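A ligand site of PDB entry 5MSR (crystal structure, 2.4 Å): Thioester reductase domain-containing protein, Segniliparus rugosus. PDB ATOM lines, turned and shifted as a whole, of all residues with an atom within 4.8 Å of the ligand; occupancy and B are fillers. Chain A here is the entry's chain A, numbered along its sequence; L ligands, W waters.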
ATOM      1  N   SER A 723      11.779  31.505 -13.983  1.00  0.00           N
ATOM      2  CA  SER A 723      10.562  30.861 -13.444  1.00  0.00           C
ATOM      3  C   SER A 723       9.724  30.104 -14.488  1.00  0.00           C
ATOM      4  O   SER A 723       9.152  29.062 -14.178  1.00  0.00           O
ATOM      5  CB  SER A 723       9.655  31.861 -12.719  1.00  0.00           C
ATOM      6  OG  SER A 723       9.018  31.295 -11.593  1.00  0.00           O
ATOM      7  N   GLY A 799       4.025  27.058  -1.003  1.00  0.00           N
ATOM      8  CA  GLY A 799       5.350  26.479  -0.817  1.00  0.00           C
ATOM      9  C   GLY A 799       5.409  25.147  -0.085  1.00  0.00           C
ATOM     10  O   GLY A 799       6.460  24.783   0.438  1.00  0.00           O
ATOM     11  N   SER A 800       4.308  24.397  -0.087  1.00  0.00           N
ATOM     12  CA  SER A 800       4.198  23.161   0.720  1.00  0.00           C
ATOM     13  C   SER A 800       5.162  22.031   0.340  1.00  0.00           C
ATOM     14  O   SER A 800       5.460  21.186   1.175  1.00  0.00           O
ATOM     15  CB  SER A 800       2.769  22.620   0.693  1.00  0.00           C
ATOM     16  OG  SER A 800       2.455  22.105  -0.591  1.00  0.00           O
ATOM     17  N   ASN A 801       5.613  21.985  -0.920  1.00  0.00           N
ATOM     18  CA  ASN A 801       6.632  20.987  -1.317  1.00  0.00           C
ATOM     19  C   ASN A 801       8.059  21.478  -1.084  1.00  0.00           C
ATOM     20  O   ASN A 801       9.011  20.735  -1.326  1.00  0.00           O
ATOM     21  CB  ASN A 801       6.438  20.536  -2.768  1.00  0.00           C
ATOM     22  CG  ASN A 801       6.715  21.631  -3.770  1.00  0.00           C
ATOM     23  OD1 ASN A 801       6.057  22.676  -3.752  1.00  0.00           O
ATOM     24  ND2 ASN A 801       7.678  21.413  -4.652  1.00  0.00           N
ATOM     25  N   GLY A 802       8.220  22.711  -0.615  1.00  0.00           N
ATOM     26  CA  GLY A 802       9.525  23.225  -0.179  1.00  0.00           C
ATOM     27  C   GLY A 802      10.015  22.614   1.122  1.00  0.00           C
ATOM     28  O   GLY A 802       9.368  21.733   1.697  1.00  0.00           O
ATOM     29  N   TRP A 803      11.177  23.080   1.578  1.00  0.00           N
ATOM     30  CA  TRP A 803      11.824  22.521   2.766  1.00  0.00           C
ATOM     31  C   TRP A 803      11.035  22.854   4.038  1.00  0.00           C
ATOM     32  O   TRP A 803      10.677  21.962   4.788  1.00  0.00           O
ATOM     33  CB  TRP A 803      13.274  23.005   2.887  1.00  0.00           C
ATOM     34  CG  TRP A 803      13.890  22.678   4.188  1.00  0.00           C
ATOM     35  CD1 TRP A 803      14.487  23.556   5.048  1.00  0.00           C
ATOM     36  CD2 TRP A 803      13.950  21.399   4.820  1.00  0.00           C
ATOM     37  NE1 TRP A 803      14.936  22.901   6.166  1.00  0.00           N
ATOM     38  CE2 TRP A 803      14.609  21.574   6.056  1.00  0.00           C
ATOM     39  CE3 TRP A 803      13.515  20.115   4.463  1.00  0.00           C
ATOM     40  CZ2 TRP A 803      14.855  20.515   6.939  1.00  0.00           C
ATOM     41  CZ3 TRP A 803      13.760  19.056   5.347  1.00  0.00           C
ATOM     42  CH2 TRP A 803      14.420  19.266   6.570  1.00  0.00           C
ATOM     43  N   LEU A 804      10.794  24.141   4.274  1.00  0.00           N
ATOM     44  CA  LEU A 804      10.025  24.559   5.448  1.00  0.00           C
ATOM     45  C   LEU A 804       8.546  24.239   5.280  1.00  0.00           C
ATOM     46  O   LEU A 804       7.913  23.738   6.200  1.00  0.00           O
ATOM     47  CB  LEU A 804      10.210  26.058   5.733  1.00  0.00           C
ATOM     48  CG  LEU A 804       9.389  26.666   6.883  1.00  0.00           C
ATOM     49  CD1 LEU A 804       9.607  25.940   8.204  1.00  0.00           C
ATOM     50  CD2 LEU A 804       9.740  28.135   7.025  1.00  0.00           C
ATOM     51  N   GLY A 805       8.005  24.553   4.096  1.00  0.00           N
ATOM     52  CA  GLY A 805       6.571  24.431   3.828  1.00  0.00           C
ATOM     53  C   GLY A 805       5.941  23.066   4.071  1.00  0.00           C
ATOM     54  O   GLY A 805       4.777  23.000   4.486  1.00  0.00           O
ATOM     55  N   ARG A 828       3.052  23.779  -7.965  1.00  0.00           N
ATOM     56  CA  ARG A 828       3.250  23.904  -9.416  1.00  0.00           C
ATOM     57  C   ARG A 828       3.254  22.525 -10.073  1.00  0.00           C
ATOM     58  O   ARG A 828       3.881  21.591  -9.570  1.00  0.00           O
ATOM     59  CB  ARG A 828       4.556  24.636  -9.725  1.00  0.00           C
ATOM     60  CG  ARG A 828       4.544  26.095  -9.306  1.00  0.00           C
ATOM     61  CD  ARG A 828       5.573  26.923 -10.056  1.00  0.00           C
ATOM     62  NE  ARG A 828       6.947  26.609  -9.670  1.00  0.00           N
ATOM     63  CZ  ARG A 828       8.024  27.262 -10.097  1.00  0.00           C
ATOM     64  NH1 ARG A 828       7.928  28.286 -10.956  1.00  0.00           N
ATOM     65  NH2 ARG A 828       9.233  26.885  -9.670  1.00  0.00           N
ATOM     66  N   ARG A 838       4.022  15.519  -6.884  1.00  0.00           N
ATOM     67  CA  ARG A 838       5.222  16.279  -6.489  1.00  0.00           C
ATOM     68  C   ARG A 838       5.300  16.513  -4.962  1.00  0.00           C
ATOM     69  O   ARG A 838       6.373  16.379  -4.373  1.00  0.00           O
ATOM     70  CB  ARG A 838       5.287  17.615  -7.216  1.00  0.00           C
ATOM     71  CG  ARG A 838       5.627  17.495  -8.690  1.00  0.00           C
ATOM     72  CD  ARG A 838       5.830  18.861  -9.326  1.00  0.00           C
ATOM     73  NE  ARG A 838       7.110  19.426  -8.901  1.00  0.00           N
ATOM     74  CZ  ARG A 838       7.300  20.630  -8.353  1.00  0.00           C
ATOM     75  NH1 ARG A 838       6.309  21.514  -8.165  1.00  0.00           N
ATOM     76  NH2 ARG A 838       8.530  20.970  -8.001  1.00  0.00           N
ATOM     77  N   GLY A 867      -1.202  25.214  -9.505  1.00  0.00           N
ATOM     78  CA  GLY A 867      -1.245  26.666  -9.619  1.00  0.00           C
ATOM     79  C   GLY A 867       0.116  27.305  -9.646  1.00  0.00           C
ATOM     80  O   GLY A 867       1.134  26.631  -9.704  1.00  0.00           O
ATOM     81  N   ASP A 868       0.119  28.637  -9.626  1.00  0.00           N
ATOM     82  CA  ASP A 868       1.334  29.440  -9.702  1.00  0.00           C
ATOM     83  C   ASP A 868       0.985  30.840  -9.195  1.00  0.00           C
ATOM     84  O   ASP A 868       0.216  31.558  -9.844  1.00  0.00           O
ATOM     85  CB  ASP A 868       1.845  29.498 -11.159  1.00  0.00           C
ATOM     86  CG  ASP A 868       3.193  30.204 -11.283  1.00  0.00           C
ATOM     87  OD1 ASP A 868       3.419  31.249 -10.644  1.00  0.00           O
ATOM     88  OD2 ASP A 868       4.046  29.698 -12.036  1.00  0.00           O
ATOM     89  N   PHE A 869       1.569  31.238  -8.055  1.00  0.00           N
ATOM     90  CA  PHE A 869       1.187  32.513  -7.419  1.00  0.00           C
ATOM     91  C   PHE A 869       1.666  33.778  -8.148  1.00  0.00           C
ATOM     92  O   PHE A 869       1.137  34.858  -7.885  1.00  0.00           O
ATOM     93  CB  PHE A 869       1.511  32.563  -5.914  1.00  0.00           C
ATOM     94  CG  PHE A 869       2.911  32.151  -5.549  1.00  0.00           C
ATOM     95  CD1 PHE A 869       4.010  32.900  -5.940  1.00  0.00           C
ATOM     96  CD2 PHE A 869       3.125  31.016  -4.780  1.00  0.00           C
ATOM     97  CE1 PHE A 869       5.298  32.512  -5.584  1.00  0.00           C
ATOM     98  CE2 PHE A 869       4.411  30.634  -4.407  1.00  0.00           C
ATOM     99  CZ  PHE A 869       5.492  31.386  -4.814  1.00  0.00           C
ATOM    100  N   SER A 870       2.641  33.652  -9.050  1.00  0.00           N
ATOM    101  CA  SER A 870       3.060  34.787  -9.901  1.00  0.00           C
ATOM    102  C   SER A 870       1.997  35.165 -10.961  1.00  0.00           C
ATOM    103  O   SER A 870       1.926  36.320 -11.367  1.00  0.00           O
ATOM    104  CB  SER A 870       4.401  34.513 -10.572  1.00  0.00           C
ATOM    105  OG  SER A 870       4.281  33.514 -11.560  1.00  0.00           O
ATOM    106  N   SER A 894       4.629  30.738   2.416  1.00  0.00           N
ATOM    107  CA  SER A 894       6.005  30.239   2.523  1.00  0.00           C
ATOM    108  C   SER A 894       6.699  30.062   1.165  1.00  0.00           C
ATOM    109  O   SER A 894       7.914  29.854   1.117  1.00  0.00           O
ATOM    110  CB  SER A 894       5.999  28.893   3.276  1.00  0.00           C
ATOM    111  OG  SER A 894       7.317  28.397   3.453  1.00  0.00           O
ATOM    112  N   GLY A 895       5.949  30.151   0.070  1.00  0.00           N
ATOM    113  CA  GLY A 895       6.496  29.933  -1.253  1.00  0.00           C
ATOM    114  C   GLY A 895       7.231  31.144  -1.820  1.00  0.00           C
ATOM    115  O   GLY A 895       6.777  32.278  -1.660  1.00  0.00           O
ATOM    116  N   ALA A 896       8.345  30.877  -2.485  1.00  0.00           N
ATOM    117  CA  ALA A 896       9.178  31.909  -3.095  1.00  0.00           C
ATOM    118  C   ALA A 896      10.281  31.235  -3.907  1.00  0.00           C
ATOM    119  O   ALA A 896      10.574  30.053  -3.700  1.00  0.00           O
ATOM    120  CB  ALA A 896       9.801  32.799  -2.042  1.00  0.00           C
ATOM    121  N   LEU A 897      10.891  31.985  -4.812  1.00  0.00           N
ATOM    122  CA  LEU A 897      12.086  31.547  -5.506  1.00  0.00           C
ATOM    123  C   LEU A 897      13.279  31.958  -4.662  1.00  0.00           C
ATOM    124  O   LEU A 897      13.673  33.123  -4.642  1.00  0.00           O
ATOM    125  CB  LEU A 897      12.166  32.122  -6.922  1.00  0.00           C
ATOM    126  CG  LEU A 897      13.385  31.740  -7.784  1.00  0.00           C
ATOM    127  CD1 LEU A 897      13.768  30.282  -7.688  1.00  0.00           C
ATOM    128  CD2 LEU A 897      13.115  32.102  -9.237  1.00  0.00           C
ATOM    129  N   VAL A 898      13.819  30.982  -3.926  1.00  0.00           N
ATOM    130  CA  VAL A 898      14.903  31.198  -2.963  1.00  0.00           C
ATOM    131  C   VAL A 898      16.215  30.923  -3.669  1.00  0.00           C
ATOM    132  O   VAL A 898      16.681  29.786  -3.714  1.00  0.00           O
ATOM    133  CB  VAL A 898      14.731  30.306  -1.722  1.00  0.00           C
ATOM    134  CG1 VAL A 898      15.831  30.572  -0.694  1.00  0.00           C
ATOM    135  CG2 VAL A 898      13.360  30.521  -1.090  1.00  0.00           C
ATOM    136  N   PRO A 910       8.017  35.862  -9.070  1.00  0.00           N
ATOM    137  CA  PRO A 910       7.689  34.931  -7.983  1.00  0.00           C
ATOM    138  C   PRO A 910       7.488  35.621  -6.622  1.00  0.00           C
ATOM    139  O   PRO A 910       6.464  35.407  -5.985  1.00  0.00           O
ATOM    140  CB  PRO A 910       8.889  33.976  -7.937  1.00  0.00           C
ATOM    141  CG  PRO A 910       9.638  34.181  -9.201  1.00  0.00           C
ATOM    142  CD  PRO A 910       9.312  35.542  -9.699  1.00  0.00           C
ATOM    143  N   LEU A 933       6.686  34.429   5.124  1.00  0.00           N
ATOM    144  CA  LEU A 933       8.061  34.034   5.379  1.00  0.00           C
ATOM    145  C   LEU A 933       8.991  35.006   4.683  1.00  0.00           C
ATOM    146  O   LEU A 933       8.759  35.365   3.531  1.00  0.00           O
ATOM    147  CB  LEU A 933       8.330  32.600   4.910  1.00  0.00           C
ATOM    148  CG  LEU A 933       8.023  31.457   5.882  1.00  0.00           C
ATOM    149  CD1 LEU A 933       9.056  31.435   7.002  1.00  0.00           C
ATOM    150  CD2 LEU A 933       6.606  31.534   6.453  1.00  0.00           C
ATOM    151  N   SER A 934      10.034  35.424   5.382  1.00  0.00           N
ATOM    152  CA  SER A 934      11.000  36.376   4.874  1.00  0.00           C
ATOM    153  C   SER A 934      12.411  35.945   5.279  1.00  0.00           C
ATOM    154  O   SER A 934      12.613  34.787   5.650  1.00  0.00           O
ATOM    155  CB  SER A 934      10.668  37.779   5.376  1.00  0.00           C
ATOM    156  OG  SER A 934      11.456  38.761   4.704  1.00  0.00           O
ATOM    157  N   THR A 935      13.377  36.863   5.215  1.00  0.00           N
ATOM    158  CA  THR A 935      14.789  36.511   5.335  1.00  0.00           C
ATOM    159  C   THR A 935      15.595  37.610   6.038  1.00  0.00           C
ATOM    160  O   THR A 935      15.241  38.783   5.968  1.00  0.00           O
ATOM    161  CB  THR A 935      15.401  36.236   3.944  1.00  0.00           C
ATOM    162  OG1 THR A 935      16.802  35.979   4.050  1.00  0.00           O
ATOM    163  CG2 THR A 935      15.190  37.425   2.998  1.00  0.00           C
ATOM    164  N   TYR A 970      17.658  38.525  -3.969  1.00  0.00           N
ATOM    165  CA  TYR A 970      16.819  37.771  -3.030  1.00  0.00           C
ATOM    166  C   TYR A 970      16.334  38.671  -1.893  1.00  0.00           C
ATOM    167  O   TYR A 970      15.121  38.784  -1.659  1.00  0.00           O
ATOM    168  CB  TYR A 970      17.567  36.560  -2.477  1.00  0.00           C
ATOM    169  CG  TYR A 970      16.768  35.746  -1.465  1.00  0.00           C
ATOM    170  CD1 TYR A 970      15.506  35.246  -1.787  1.00  0.00           C
ATOM    171  CD2 TYR A 970      17.286  35.493  -0.195  1.00  0.00           C
ATOM    172  CE1 TYR A 970      14.769  34.511  -0.863  1.00  0.00           C
ATOM    173  CE2 TYR A 970      16.562  34.755   0.732  1.00  0.00           C
ATOM    174  CZ  TYR A 970      15.298  34.274   0.396  1.00  0.00           C
ATOM    175  OH  TYR A 970      14.590  33.558   1.305  1.00  0.00           O
ATOM    176  N   LYS A 974      12.331  39.838  -1.227  1.00  0.00           N
ATOM    177  CA  LYS A 974      11.619  39.528   0.027  1.00  0.00           C
ATOM    178  C   LYS A 974      11.259  40.804   0.797  1.00  0.00           C
ATOM    179  O   LYS A 974      10.158  40.907   1.352  1.00  0.00           O
ATOM    180  CB  LYS A 974      12.471  38.589   0.904  1.00  0.00           C
ATOM    181  CG  LYS A 974      12.752  37.219   0.294  1.00  0.00           C
ATOM    182  CD  LYS A 974      11.514  36.419  -0.091  1.00  0.00           C
ATOM    183  CE  LYS A 974      10.602  36.129   1.086  1.00  0.00           C
ATOM    184  NZ  LYS A 974       9.425  35.301   0.702  1.00  0.00           N
ATOM    185  N   SER A 997      13.744  34.036   8.404  1.00  0.00           N
ATOM    186  CA  SER A 997      14.377  32.752   8.691  1.00  0.00           C
ATOM    187  C   SER A 997      15.365  32.357   7.605  1.00  0.00           C
ATOM    188  O   SER A 997      14.988  32.259   6.441  1.00  0.00           O
ATOM    189  CB  SER A 997      13.309  31.663   8.792  1.00  0.00           C
ATOM    190  OG  SER A 997      12.492  31.652   7.631  1.00  0.00           O
ATOM    191  N   ASN A1011      17.590  19.678   4.405  1.00  0.00           N
ATOM    192  CA  ASN A1011      17.649  20.494   3.188  1.00  0.00           C
ATOM    193  C   ASN A1011      18.979  20.216   2.498  1.00  0.00           C
ATOM    194  O   ASN A1011      20.011  20.762   2.866  1.00  0.00           O
ATOM    195  CB  ASN A1011      17.462  21.975   3.552  1.00  0.00           C
ATOM    196  CG  ASN A1011      17.179  22.857   2.343  1.00  0.00           C
ATOM    197  OD1 ASN A1011      16.910  22.356   1.261  1.00  0.00           O
ATOM    198  ND2 ASN A1011      17.187  24.175   2.531  1.00  0.00           N
HETATM  199  P1  LIG L   1      12.333  26.099  -0.900  1.00  0.00           P
HETATM  200  O1  LIG L   1      12.609  24.791  -0.204  1.00  0.00           O
HETATM  201  O2  LIG L   1      13.172  26.523  -2.082  1.00  0.00           O
HETATM  202  O3  LIG L   1      10.786  26.055  -1.327  1.00  0.00           O
HETATM  203  C1  LIG L   1      10.211  27.048  -2.163  1.00  0.00           C
HETATM  204  C2  LIG L   1       8.763  26.683  -2.440  1.00  0.00           C
HETATM  205  O4  LIG L   1       8.124  27.710  -3.224  1.00  0.00           O
HETATM  206  C3  LIG L   1       8.646  25.401  -3.246  1.00  0.00           C
HETATM  207  O5  LIG L   1       7.503  24.665  -2.810  1.00  0.00           O
HETATM  208  C4  LIG L   1       8.467  25.935  -4.650  1.00  0.00           C
HETATM  209  O6  LIG L   1       7.875  25.021  -5.558  1.00  0.00           O
HETATM  210  C5  LIG L   1       7.547  27.095  -4.386  1.00  0.00           C
HETATM  211  N1  LIG L   1       7.457  28.050  -5.518  1.00  0.00           N
HETATM  212  C6  LIG L   1       8.484  28.719  -6.077  1.00  0.00           C
HETATM  213  N2  LIG L   1       8.033  29.519  -7.082  1.00  0.00           N
HETATM  214  C7  LIG L   1       6.700  29.368  -7.160  1.00  0.00           C
HETATM  215  C8  LIG L   1       5.606  29.917  -7.984  1.00  0.00           C
HETATM  216  N3  LIG L   1       5.868  30.816  -8.964  1.00  0.00           N
HETATM  217  N4  LIG L   1       4.337  29.495  -7.750  1.00  0.00           N
HETATM  218  C9  LIG L   1       4.058  28.582  -6.774  1.00  0.00           C
HETATM  219  N5  LIG L   1       5.016  28.043  -5.988  1.00  0.00           N
HETATM  220  C10 LIG L   1       6.324  28.393  -6.120  1.00  0.00           C
HETATM  221  O7  LIG L   1      12.364  27.322   0.152  1.00  0.00           O
HETATM  222  P2  LIG L   1      12.283  27.113   1.748  1.00  0.00           P
HETATM  223  O8  LIG L   1      13.667  26.691   2.176  1.00  0.00           O
HETATM  224  O9  LIG L   1      11.069  26.266   2.058  1.00  0.00           O
HETATM  225  O10 LIG L   1      12.015  28.617   2.265  1.00  0.00           O
HETATM  226  C11 LIG L   1      10.768  28.988   2.845  1.00  0.00           C
HETATM  227  C12 LIG L   1      10.567  30.503   2.963  1.00  0.00           C
HETATM  228  O11 LIG L   1      11.438  31.080   3.955  1.00  0.00           O
HETATM  229  C13 LIG L   1      10.820  31.255   1.651  1.00  0.00           C
HETATM  230  O12 LIG L   1       9.715  32.116   1.368  1.00  0.00           O
HETATM  231  C14 LIG L   1      12.100  32.032   1.895  1.00  0.00           C
HETATM  232  O13 LIG L   1      12.136  33.285   1.201  1.00  0.00           O
HETATM  233  C15 LIG L   1      12.146  32.196   3.413  1.00  0.00           C
HETATM  234  N6  LIG L   1      13.528  32.201   3.898  1.00  0.00           N
HETATM  235  P3  LIG L   1       8.643  24.464  -6.867  1.00  0.00           P
HETATM  236  O14 LIG L   1       9.758  25.403  -7.259  1.00  0.00           O
HETATM  237  O15 LIG L   1       9.147  23.129  -6.394  1.00  0.00           O
HETATM  238  O16 LIG L   1       7.511  24.391  -7.873  1.00  0.00           O
HETATM  239  O   HOH W   1       9.713  30.668  -9.199  1.00  0.00           O
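An oxygen (O5) of the ligand lies within hydrogen-bond range of the backbone carbonyl oxygen of Gly 799 (3.4 Å). O of Ser 894 sits at hydrogen-bond distance from O12 of the ligand, at 2.9 Å. N of Leu 804 is in hydrogen-bond range of O9 of the ligand, 3.1 Å away. OH of Tyr 970 is in hydrogen-bond range of O13 of the ligand (2.5 Å). NZ of Lys 974 is in hydrogen-bond range of O12 of the ligand (3.3 Å). A nitrogen (N3) of the ligand is in hydrogen-bond range of the side-chain carboxylate (OD1) of Asp 868, at 3.0 Å. O14 of the ligand lies within salt-bridge range of NH2 of Arg 828 (2.9 Å). The backbone NH (N) of Trp 803 sits at hydrogen-bond distance from an oxygen (O1) of the ligand. The backbone NH (N) of Ala 896 lies within hydrogen-bond range of an oxygen (O4) of the ligand (3.3 Å). The backbone NH of Phe 869 lies within hydrogen-bond range of a nitrogen (N4) of the ligand (3.3 Å). The backbone NH (N) of Gly 802 sits at hydrogen-bond distance from an oxygen (O5) of the ligand (3.0 Å). NH2 of Arg 838 lies within salt-bridge range of O15 of the ligand (2.8 Å). An oxygen (O5) of the ligand sits at hydrogen-bond distance from the side-chain amide oxygen (OD1) of Asn 801, 2.6 Å away.
OG of Ser 723 lies within hydrogen-bond range of NH1 of Arg 828, 3.3 Å away. NH1 of Arg 838 sits at hydrogen-bond distance from O of Arg 828 (2.8 Å). ND2 of Asn 801 lies close to NH2 of Arg 838, at 3.5 Å. The side-chain amino group (NZ) of Lys 974 sits at hydrogen-bond distance from the backbone carbonyl oxygen (O) of Leu 933 (2.9 Å). The backbone carbonyl oxygen of Ser 934 lies within hydrogen-bond range of the backbone NH of Ser 997, at 3.1 Å. OD1 of Asp 868 sits at hydrogen-bond distance from OG of Ser 870 (2.6 Å).
The backbone carbonyl oxygen (O) of Ser 934 lies close to a nitrogen (N6) of the ligand, at 3.3 Å. N6 of the ligand lies close to O of Ser 997 (2.9 Å). Gly 895 touches the ligand (CA to O4, 3.4 Å). CG2 of Val 898 touches O7 of the ligand, 3.6 Å away. CB of Leu 933 touches O11 of the ligand, at 3.6 Å. Hydrophobic or aromatic side chains within 4 Å of the ligand: Trp 803, Leu 804, Phe 869, Ala 896, Val 898, Leu 933 and Tyr 970. Along chain A the residues within 4 Å of the ligand span positions 799 to 997. The nearest printed residue that does not touch the ligand is Gly 805 (4.1 Å).
Water W1 lies within hydrogen-bond range of the side-chain hydroxyl (OG) of Ser 723 (2.6 Å), a nitrogen (N2) of the ligand (2.9 Å) and the guanidinium group (NH1) of Arg 828 (3.5 Å).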
